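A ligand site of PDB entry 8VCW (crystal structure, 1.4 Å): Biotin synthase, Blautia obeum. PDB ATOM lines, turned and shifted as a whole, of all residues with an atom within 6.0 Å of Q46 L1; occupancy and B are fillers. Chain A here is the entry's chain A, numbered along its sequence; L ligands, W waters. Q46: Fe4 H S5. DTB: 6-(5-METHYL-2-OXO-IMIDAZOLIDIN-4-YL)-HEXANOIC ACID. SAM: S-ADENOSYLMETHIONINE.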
ATOM      1  N   ASP A  50       0.397 -15.638 -13.331  1.00  0.00           N
ATOM      2  CA  ASP A  50       1.243 -14.508 -12.955  1.00  0.00           C
ATOM      3  C   ASP A  50       0.418 -13.523 -12.135  1.00  0.00           C
ATOM      4  O   ASP A  50      -0.699 -13.149 -12.524  1.00  0.00           O
ATOM      5  CB  ASP A  50       1.732 -13.805 -14.226  1.00  0.00           C
ATOM      6  CG  ASP A  50       2.804 -12.779 -13.905  1.00  0.00           C
ATOM      7  OD1 ASP A  50       3.910 -13.220 -13.533  1.00  0.00           O
ATOM      8  OD2 ASP A  50       2.531 -11.575 -13.967  1.00  0.00           O
ATOM      9  N   CYS A  52       0.416  -9.750 -10.303  1.00  0.00           N
ATOM     10  CA  CYS A  52       1.103  -8.484 -10.205  1.00  0.00           C
ATOM     11  C   CYS A  52       0.418  -7.579  -9.193  1.00  0.00           C
ATOM     12  O   CYS A  52      -0.644  -7.908  -8.641  1.00  0.00           O
ATOM     13  CB  CYS A  52       1.163  -7.788 -11.561  1.00  0.00           C
ATOM     14  SG  CYS A  52      -0.480  -7.398 -12.270  1.00  0.00           S
ATOM     15  N   SER A  53       1.088  -6.461  -8.868  1.00  0.00           N
ATOM     16  CA  SER A  53       0.624  -5.556  -7.827  1.00  0.00           C
ATOM     17  C   SER A  53       1.037  -4.146  -8.217  1.00  0.00           C
ATOM     18  O   SER A  53       1.957  -3.954  -9.008  1.00  0.00           O
ATOM     19  CB  SER A  53       1.280  -5.933  -6.479  1.00  0.00           C
ATOM     20  OG  SER A  53       2.706  -5.970  -6.628  1.00  0.00           O
ATOM     21  N   ILE A  54       0.356  -3.184  -7.643  1.00  0.00           N
ATOM     22  CA  ILE A  54       0.521  -1.790  -8.022  1.00  0.00           C
ATOM     23  C   ILE A  54       0.569  -0.895  -6.800  1.00  0.00           C
ATOM     24  O   ILE A  54      -0.021  -1.212  -5.756  1.00  0.00           O
ATOM     25  CB  ILE A  54      -0.590  -1.340  -9.011  1.00  0.00           C
ATOM     26  CG1 ILE A  54      -1.962  -1.263  -8.349  1.00  0.00           C
ATOM     27  CG2 ILE A  54      -0.629  -2.242 -10.252  1.00  0.00           C
ATOM     28  CD1 ILE A  54      -3.077  -0.865  -9.336  1.00  0.00           C
ATOM     29  N   ARG A 104       5.387  -9.387  -9.734  1.00  0.00           N
ATOM     30  CA  ARG A 104       5.854  -8.115 -10.230  1.00  0.00           C
ATOM     31  C   ARG A 104       5.056  -6.971  -9.605  1.00  0.00           C
ATOM     32  O   ARG A 104       3.956  -7.171  -9.044  1.00  0.00           O
ATOM     33  CB  ARG A 104       5.844  -8.055 -11.752  1.00  0.00           C
ATOM     34  CG  ARG A 104       4.474  -8.131 -12.391  1.00  0.00           C
ATOM     35  CD  ARG A 104       4.543  -8.558 -13.847  1.00  0.00           C
ATOM     36  NE  ARG A 104       4.879  -9.963 -13.980  1.00  0.00           N
ATOM     37  CZ  ARG A 104       6.085 -10.429 -14.237  1.00  0.00           C
ATOM     38  NH1 ARG A 104       7.096  -9.629 -14.557  1.00  0.00           N
ATOM     39  NH2 ARG A 104       6.286 -11.762 -14.157  1.00  0.00           N
ATOM     40  N   PHE A 105       5.656  -5.782  -9.643  1.00  0.00           N
ATOM     41  CA  PHE A 105       5.157  -4.595  -8.958  1.00  0.00           C
ATOM     42  C   PHE A 105       5.318  -3.367  -9.838  1.00  0.00           C
ATOM     43  O   PHE A 105       6.387  -3.151 -10.439  1.00  0.00           O
ATOM     44  CB  PHE A 105       5.999  -4.412  -7.668  1.00  0.00           C
ATOM     45  CG  PHE A 105       5.714  -3.167  -6.890  1.00  0.00           C
ATOM     46  CD1 PHE A 105       4.522  -3.022  -6.238  1.00  0.00           C
ATOM     47  CD2 PHE A 105       6.630  -2.106  -6.862  1.00  0.00           C
ATOM     48  CE1 PHE A 105       4.261  -1.885  -5.497  1.00  0.00           C
ATOM     49  CE2 PHE A 105       6.374  -0.968  -6.130  1.00  0.00           C
ATOM     50  CZ  PHE A 105       5.189  -0.858  -5.466  1.00  0.00           C
ATOM     51  N   SER A 106       4.290  -2.515  -9.861  1.00  0.00           N
ATOM     52  CA  SER A 106       4.268  -1.361 -10.747  1.00  0.00           C
ATOM     53  C   SER A 106       4.038  -0.060  -9.975  1.00  0.00           C
ATOM     54  O   SER A 106       3.216  -0.006  -9.061  1.00  0.00           O
ATOM     55  CB  SER A 106       3.097  -1.511 -11.713  1.00  0.00           C
ATOM     56  OG  SER A 106       3.195  -0.507 -12.702  1.00  0.00           O
ATOM     57  N   ILE A 107       4.697   1.021 -10.407  1.00  0.00           N
ATOM     58  CA  ILE A 107       4.355   2.386  -9.989  1.00  0.00           C
ATOM     59  C   ILE A 107       3.434   2.950 -11.044  1.00  0.00           C
ATOM     60  O   ILE A 107       3.763   2.989 -12.233  1.00  0.00           O
ATOM     61  CB  ILE A 107       5.581   3.272  -9.868  1.00  0.00           C
ATOM     62  CG1 ILE A 107       6.664   2.658  -8.958  1.00  0.00           C
ATOM     63  CG2 ILE A 107       5.124   4.650  -9.388  1.00  0.00           C
ATOM     64  CD1 ILE A 107       7.977   3.533  -8.974  1.00  0.00           C
ATOM     65  N   VAL A 108       2.237   3.352 -10.626  1.00  0.00           N
ATOM     66  CA  VAL A 108       1.203   3.882 -11.520  1.00  0.00           C
ATOM     67  C   VAL A 108       0.932   5.335 -11.162  1.00  0.00           C
ATOM     68  O   VAL A 108       0.623   5.624 -10.004  1.00  0.00           O
ATOM     69  CB  VAL A 108      -0.091   3.094 -11.323  1.00  0.00           C
ATOM     70  CG1 VAL A 108      -1.165   3.614 -12.278  1.00  0.00           C
ATOM     71  CG2 VAL A 108       0.161   1.622 -11.553  1.00  0.00           C
ATOM     72  N   LEU A 137       9.499  -5.697 -12.091  1.00  0.00           N
ATOM     73  CA  LEU A 137       9.092  -4.287 -12.060  1.00  0.00           C
ATOM     74  C   LEU A 137       8.377  -3.861 -13.319  1.00  0.00           C
ATOM     75  O   LEU A 137       8.774  -4.206 -14.431  1.00  0.00           O
ATOM     76  CB  LEU A 137      10.332  -3.380 -11.868  1.00  0.00           C
ATOM     77  CG  LEU A 137      11.058  -3.651 -10.567  1.00  0.00           C
ATOM     78  CD1 LEU A 137      12.399  -2.926 -10.543  1.00  0.00           C
ATOM     79  CD2 LEU A 137      10.217  -3.239  -9.326  1.00  0.00           C
ATOM     80  N   CYS A 138       7.292  -3.125 -13.134  1.00  0.00           N
ATOM     81  CA  CYS A 138       6.521  -2.515 -14.221  1.00  0.00           C
ATOM     82  C   CYS A 138       6.353  -1.026 -13.984  1.00  0.00           C
ATOM     83  O   CYS A 138       6.595  -0.552 -12.863  1.00  0.00           O
ATOM     84  CB  CYS A 138       5.101  -3.103 -14.284  1.00  0.00           C
ATOM     85  SG  CYS A 138       4.986  -4.940 -14.287  1.00  0.00           S
ATOM     86  N   ALA A 139       5.893  -0.310 -15.018  1.00  0.00           N
ATOM     87  CA  ALA A 139       5.550   1.111 -14.863  1.00  0.00           C
ATOM     88  C   ALA A 139       4.283   1.421 -15.650  1.00  0.00           C
ATOM     89  O   ALA A 139       4.070   0.834 -16.712  1.00  0.00           O
ATOM     90  CB  ALA A 139       6.683   2.003 -15.413  1.00  0.00           C
ATOM     91  N   SER A 140       3.468   2.353 -15.127  1.00  0.00           N
ATOM     92  CA  SER A 140       2.303   2.882 -15.853  1.00  0.00           C
ATOM     93  C   SER A 140       2.290   4.386 -15.649  1.00  0.00           C
ATOM     94  O   SER A 140       1.860   4.875 -14.593  1.00  0.00           O
ATOM     95  CB  SER A 140       1.048   2.246 -15.289  1.00  0.00           C
ATOM     96  OG  SER A 140      -0.071   2.648 -16.078  1.00  0.00           O
ATOM     97  N   SER A 159       8.216  -4.344 -17.941  1.00  0.00           N
ATOM     98  CA  SER A 159       6.923  -4.184 -18.613  1.00  0.00           C
ATOM     99  C   SER A 159       6.478  -2.743 -18.519  1.00  0.00           C
ATOM    100  O   SER A 159       6.655  -2.105 -17.470  1.00  0.00           O
ATOM    101  CB  SER A 159       5.811  -5.001 -17.956  1.00  0.00           C
ATOM    102  OG  SER A 159       6.139  -6.390 -17.984  1.00  0.00           O
ATOM    103  N   TYR A 160       5.822  -2.246 -19.553  1.00  0.00           N
ATOM    104  CA  TYR A 160       5.216  -0.923 -19.551  1.00  0.00           C
ATOM    105  C   TYR A 160       3.729  -1.086 -19.777  1.00  0.00           C
ATOM    106  O   TYR A 160       3.336  -1.796 -20.733  1.00  0.00           O
ATOM    107  CB  TYR A 160       5.828   0.017 -20.602  1.00  0.00           C
ATOM    108  CG  TYR A 160       5.374   1.429 -20.339  1.00  0.00           C
ATOM    109  CD1 TYR A 160       5.899   2.149 -19.254  1.00  0.00           C
ATOM    110  CD2 TYR A 160       4.348   2.025 -21.087  1.00  0.00           C
ATOM    111  CE1 TYR A 160       5.455   3.416 -18.961  1.00  0.00           C
ATOM    112  CE2 TYR A 160       3.911   3.302 -20.800  1.00  0.00           C
ATOM    113  CZ  TYR A 160       4.423   3.978 -19.695  1.00  0.00           C
ATOM    114  OH  TYR A 160       3.976   5.234 -19.358  1.00  0.00           O
ATOM    115  N   HIS A 161       2.940  -0.447 -18.930  1.00  0.00           N
ATOM    116  CA  HIS A 161       1.495  -0.567 -19.018  1.00  0.00           C
ATOM    117  C   HIS A 161       0.916   0.663 -19.700  1.00  0.00           C
ATOM    118  O   HIS A 161       1.189   1.814 -19.305  1.00  0.00           O
ATOM    119  CB  HIS A 161       0.958  -0.613 -17.591  1.00  0.00           C
ATOM    120  CG  HIS A 161      -0.529  -0.694 -17.521  1.00  0.00           C
ATOM    121  ND1 HIS A 161      -1.329   0.386 -17.179  1.00  0.00           N
ATOM    122  CD2 HIS A 161      -1.359  -1.737 -17.754  1.00  0.00           C
ATOM    123  CE1 HIS A 161      -2.602  -0.023 -17.218  1.00  0.00           C
ATOM    124  NE2 HIS A 161      -2.640  -1.295 -17.524  1.00  0.00           N
ATOM    125  N   CYS A 198       2.024  -4.238 -21.788  1.00  0.00           N
ATOM    126  CA  CYS A 198       0.838  -4.626 -21.050  1.00  0.00           C
ATOM    127  C   CYS A 198      -0.252  -3.641 -21.397  1.00  0.00           C
ATOM    128  O   CYS A 198      -0.119  -2.455 -21.095  1.00  0.00           O
ATOM    129  CB  CYS A 198       1.185  -4.689 -19.557  1.00  0.00           C
ATOM    130  SG  CYS A 198      -0.205  -5.240 -18.543  1.00  0.00           S
ATOM    131  N   SER A 226       0.529  -8.958 -22.414  1.00  0.00           N
ATOM    132  CA  SER A 226      -0.265  -9.027 -21.195  1.00  0.00           C
ATOM    133  C   SER A 226      -1.438  -8.124 -21.418  1.00  0.00           C
ATOM    134  O   SER A 226      -1.240  -6.971 -21.814  1.00  0.00           O
ATOM    135  CB  SER A 226       0.605  -8.552 -20.009  1.00  0.00           C
ATOM    136  OG  SER A 226      -0.130  -8.385 -18.812  1.00  0.00           O
ATOM    137  N   PRO A 228      -4.704  -6.738 -19.451  1.00  0.00           N
ATOM    138  CA  PRO A 228      -5.629  -6.559 -18.309  1.00  0.00           C
ATOM    139  C   PRO A 228      -7.033  -6.243 -18.788  1.00  0.00           C
ATOM    140  O   PRO A 228      -7.247  -5.230 -19.494  1.00  0.00           O
ATOM    141  CB  PRO A 228      -5.036  -5.377 -17.524  1.00  0.00           C
ATOM    142  CG  PRO A 228      -3.965  -4.769 -18.406  1.00  0.00           C
ATOM    143  CD  PRO A 228      -3.744  -5.633 -19.625  1.00  0.00           C
ATOM    144  N   ARG A 268      -5.334 -11.111 -18.215  1.00  0.00           N
ATOM    145  CA  ARG A 268      -5.072 -10.766 -16.841  1.00  0.00           C
ATOM    146  C   ARG A 268      -6.293 -10.088 -16.217  1.00  0.00           C
ATOM    147  O   ARG A 268      -6.799  -9.085 -16.748  1.00  0.00           O
ATOM    148  CB  ARG A 268      -3.848  -9.825 -16.855  1.00  0.00           C
ATOM    149  CG  ARG A 268      -3.384  -9.379 -15.471  1.00  0.00           C
ATOM    150  CD  ARG A 268      -2.088  -8.521 -15.572  1.00  0.00           C
ATOM    151  NE  ARG A 268      -0.966  -9.187 -16.184  1.00  0.00           N
ATOM    152  CZ  ARG A 268      -0.077  -9.933 -15.544  1.00  0.00           C
ATOM    153  NH1 ARG A 268      -0.130 -10.101 -14.218  1.00  0.00           N
ATOM    154  NH2 ARG A 268       0.891 -10.540 -16.252  1.00  0.00           N
ATOM    155  N   SER A 291      -3.375 -12.131 -12.903  1.00  0.00           N
ATOM    156  CA  SER A 291      -4.268 -11.190 -12.238  1.00  0.00           C
ATOM    157  C   SER A 291      -3.456 -10.134 -11.505  1.00  0.00           C
ATOM    158  O   SER A 291      -2.374 -10.425 -10.970  1.00  0.00           O
ATOM    159  CB  SER A 291      -5.130 -11.927 -11.225  1.00  0.00           C
ATOM    160  OG  SER A 291      -6.155 -11.056 -10.699  1.00  0.00           O
ATOM    161  N   ILE A 292      -4.008  -8.954 -11.421  1.00  0.00           N
ATOM    162  CA  ILE A 292      -3.563  -7.995 -10.407  1.00  0.00           C
ATOM    163  C   ILE A 292      -4.145  -8.449  -9.072  1.00  0.00           C
ATOM    164  O   ILE A 292      -5.301  -8.930  -8.979  1.00  0.00           O
ATOM    165  CB  ILE A 292      -4.099  -6.594 -10.717  1.00  0.00           C
ATOM    166  CG1 ILE A 292      -3.874  -6.225 -12.201  1.00  0.00           C
ATOM    167  CG2 ILE A 292      -3.405  -5.582  -9.778  1.00  0.00           C
ATOM    168  CD1 ILE A 292      -4.218  -4.725 -12.485  1.00  0.00           C
HETATM  169  S4  Q46 L   1       2.126  -3.596 -16.183  1.00  0.00           S
HETATM  170 FE1  Q46 L   1       0.587  -5.160 -16.401  1.00  0.00          FE
HETATM  171 FE3  Q46 L   1       0.676  -3.315 -14.460  1.00  0.00          FE
HETATM  172 FE2  Q46 L   1       2.721  -5.110 -14.672  1.00  0.00          FE
HETATM  173  S3  Q46 L   1       1.572  -6.879 -15.392  1.00  0.00           S
HETATM  174 FE4  Q46 L   1       0.241  -5.931 -13.823  1.00  0.00          FE
HETATM  175  S2  Q46 L   1      -1.112  -4.651 -15.019  1.00  0.00           S
HETATM  176  S1  Q46 L   1       1.595  -4.498 -12.804  1.00  0.00           S
HETATM  177  S5  Q46 L   1       0.240  -1.199 -14.029  1.00  0.00           S
HETATM  178  CN  DTB L   2      -4.970  -1.989 -15.155  1.00  0.00           C
HETATM  179  O   DTB L   2      -5.180  -2.308 -16.292  1.00  0.00           O
HETATM  180  N2  DTB L   2      -5.924  -1.527 -14.212  1.00  0.00           N
HETATM  181  CR  DTB L   2      -5.265  -1.326 -12.925  1.00  0.00           C
HETATM  182  CS  DTB L   2      -3.798  -1.361 -13.144  1.00  0.00           C
HETATM  183  N1  DTB L   2      -3.700  -1.906 -14.482  1.00  0.00           N
HETATM  184  CT  DTB L   2      -3.242   0.080 -13.288  1.00  0.00           C
HETATM  185  CE  DTB L   2      -5.861  -0.150 -12.136  1.00  0.00           C
HETATM  186  CD  DTB L   2      -7.348  -0.373 -11.827  1.00  0.00           C
HETATM  187  CG  DTB L   2      -7.957   0.897 -11.197  1.00  0.00           C
HETATM  188  CB  DTB L   2      -9.392   0.608 -10.701  1.00  0.00           C
HETATM  189  CA  DTB L   2     -10.106   1.907 -10.249  1.00  0.00           C
HETATM  190  C   DTB L   2      -9.402   2.664  -9.084  1.00  0.00           C
HETATM  191  OI1 DTB L   2      -9.445   3.944  -9.135  1.00  0.00           O
HETATM  192  OI2 DTB L   2      -8.839   2.047  -8.138  1.00  0.00           O
HETATM  193  N   SAM L   3      -2.395   8.118 -16.385  1.00  0.00           N
HETATM  194  CA  SAM L   3      -1.769   6.930 -16.980  1.00  0.00           C
HETATM  195  C   SAM L   3      -2.631   6.337 -18.074  1.00  0.00           C
HETATM  196  O   SAM L   3      -3.842   6.696 -18.179  1.00  0.00           O
HETATM  197  OXT SAM L   3      -2.115   5.500 -18.835  1.00  0.00           O
HETATM  198  CB  SAM L   3      -1.445   5.912 -15.864  1.00  0.00           C
HETATM  199  CG  SAM L   3      -2.632   5.412 -15.013  1.00  0.00           C
HETATM  200  SD  SAM L   3      -3.876   4.422 -15.871  1.00  0.00           S
HETATM  201  CE  SAM L   3      -2.929   2.909 -16.072  1.00  0.00           C
HETATM  202  C5' SAM L   3      -4.980   3.625 -14.673  1.00  0.00           C
HETATM  203  C4' SAM L   3      -5.806   2.477 -15.323  1.00  0.00           C
HETATM  204  O4' SAM L   3      -6.864   2.166 -14.434  1.00  0.00           O
HETATM  205  C3' SAM L   3      -6.486   2.958 -16.575  1.00  0.00           C
HETATM  206  O3' SAM L   3      -5.622   2.588 -17.665  1.00  0.00           O
HETATM  207  C2' SAM L   3      -7.826   2.270 -16.581  1.00  0.00           C
HETATM  208  O2' SAM L   3      -7.879   1.193 -17.491  1.00  0.00           O
HETATM  209  C1' SAM L   3      -7.977   1.675 -15.157  1.00  0.00           C
HETATM  210  N9  SAM L   3      -9.134   2.300 -14.443  1.00  0.00           N
HETATM  211  C8  SAM L   3      -9.186   3.586 -14.013  1.00  0.00           C
HETATM  212  N7  SAM L   3     -10.410   3.798 -13.523  1.00  0.00           N
HETATM  213  C5  SAM L   3     -11.142   2.631 -13.574  1.00  0.00           C
HETATM  214  C6  SAM L   3     -12.401   2.271 -13.195  1.00  0.00           C
HETATM  215  N6  SAM L   3     -13.281   3.131 -12.594  1.00  0.00           N
HETATM  216  N1  SAM L   3     -12.859   1.007 -13.402  1.00  0.00           N
HETATM  217  C2  SAM L   3     -12.024   0.117 -14.023  1.00  0.00           C
HETATM  218  N3  SAM L   3     -10.772   0.429 -14.415  1.00  0.00           N
HETATM  219  C4  SAM L   3     -10.324   1.690 -14.191  1.00  0.00           C
HETATM  220  O   HOH W   1       3.508  -7.547 -18.156  1.00  0.00           O
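The side-chain sulfur (SG) of Cys 52 binds an iron atom (FE4) of Q46 L1, 2.3 Å away. The side-chain sulfur (SG) of Cys 198 binds an iron atom (FE1) of Q46 L1, 2.3 Å away. SG of Cys 138 is bound to FE2 of Q46 L1 (2.3 Å). A sulfur (S5) of Q46 L1 sits close to the side-chain hydroxyl (OG) of Ser 106 (3.3 Å). The guanidinium group (NE) of Arg 268 sits close to a sulfur (S3) of Q46 L1 (3.5 Å). NE2 of His 161 lies within hydrogen-bond range of O of DTB L2.
SG of Cys 52 lies close to NH1 of Arg 268, 3.4 Å away. The backbone NH (N) of Cys 138 is in hydrogen-bond range of the backbone carbonyl oxygen (O) of Phe 105. The backbone carbonyl oxygen (O) of Cys 138 sits at hydrogen-bond distance from the backbone NH (N) of Ile 107 (3.5 Å). O of Ser 53 lies within hydrogen-bond range of N of Ser 106, at 2.9 Å. NE of Arg 268 is in hydrogen-bond range of OG of Ser 226 (2.9 Å). The backbone carbonyl oxygen of Arg 104 lies within hydrogen-bond range of the backbone NH of Ser 53. NE of Arg 104 lies within salt-bridge range of OD2 of Asp 50 (2.8 Å). The backbone NH of Ser 140 lies within hydrogen-bond range of the backbone carbonyl oxygen of Ile 107, 3.0 Å away.
O of Ser 53 touches S1 of Q46 L1, at 3.9 Å. CD of Arg 104 touches S3 of Q46 L1 (3.7 Å). Val 108 touches Q46 L1. Ser 140 touches Q46 L1 (CB to S5, 3.8 Å). His 161 touches Q46 L1. Of the 22 residues printed, 10 come within 4 Å of Q46 L1. The nearest printed residue that does not touch Q46 L1 is Ile 292 (4.01 Å).
Water W1 lies within hydrogen-bond range of OG of Ser 159 and S3 of Q46 L1.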
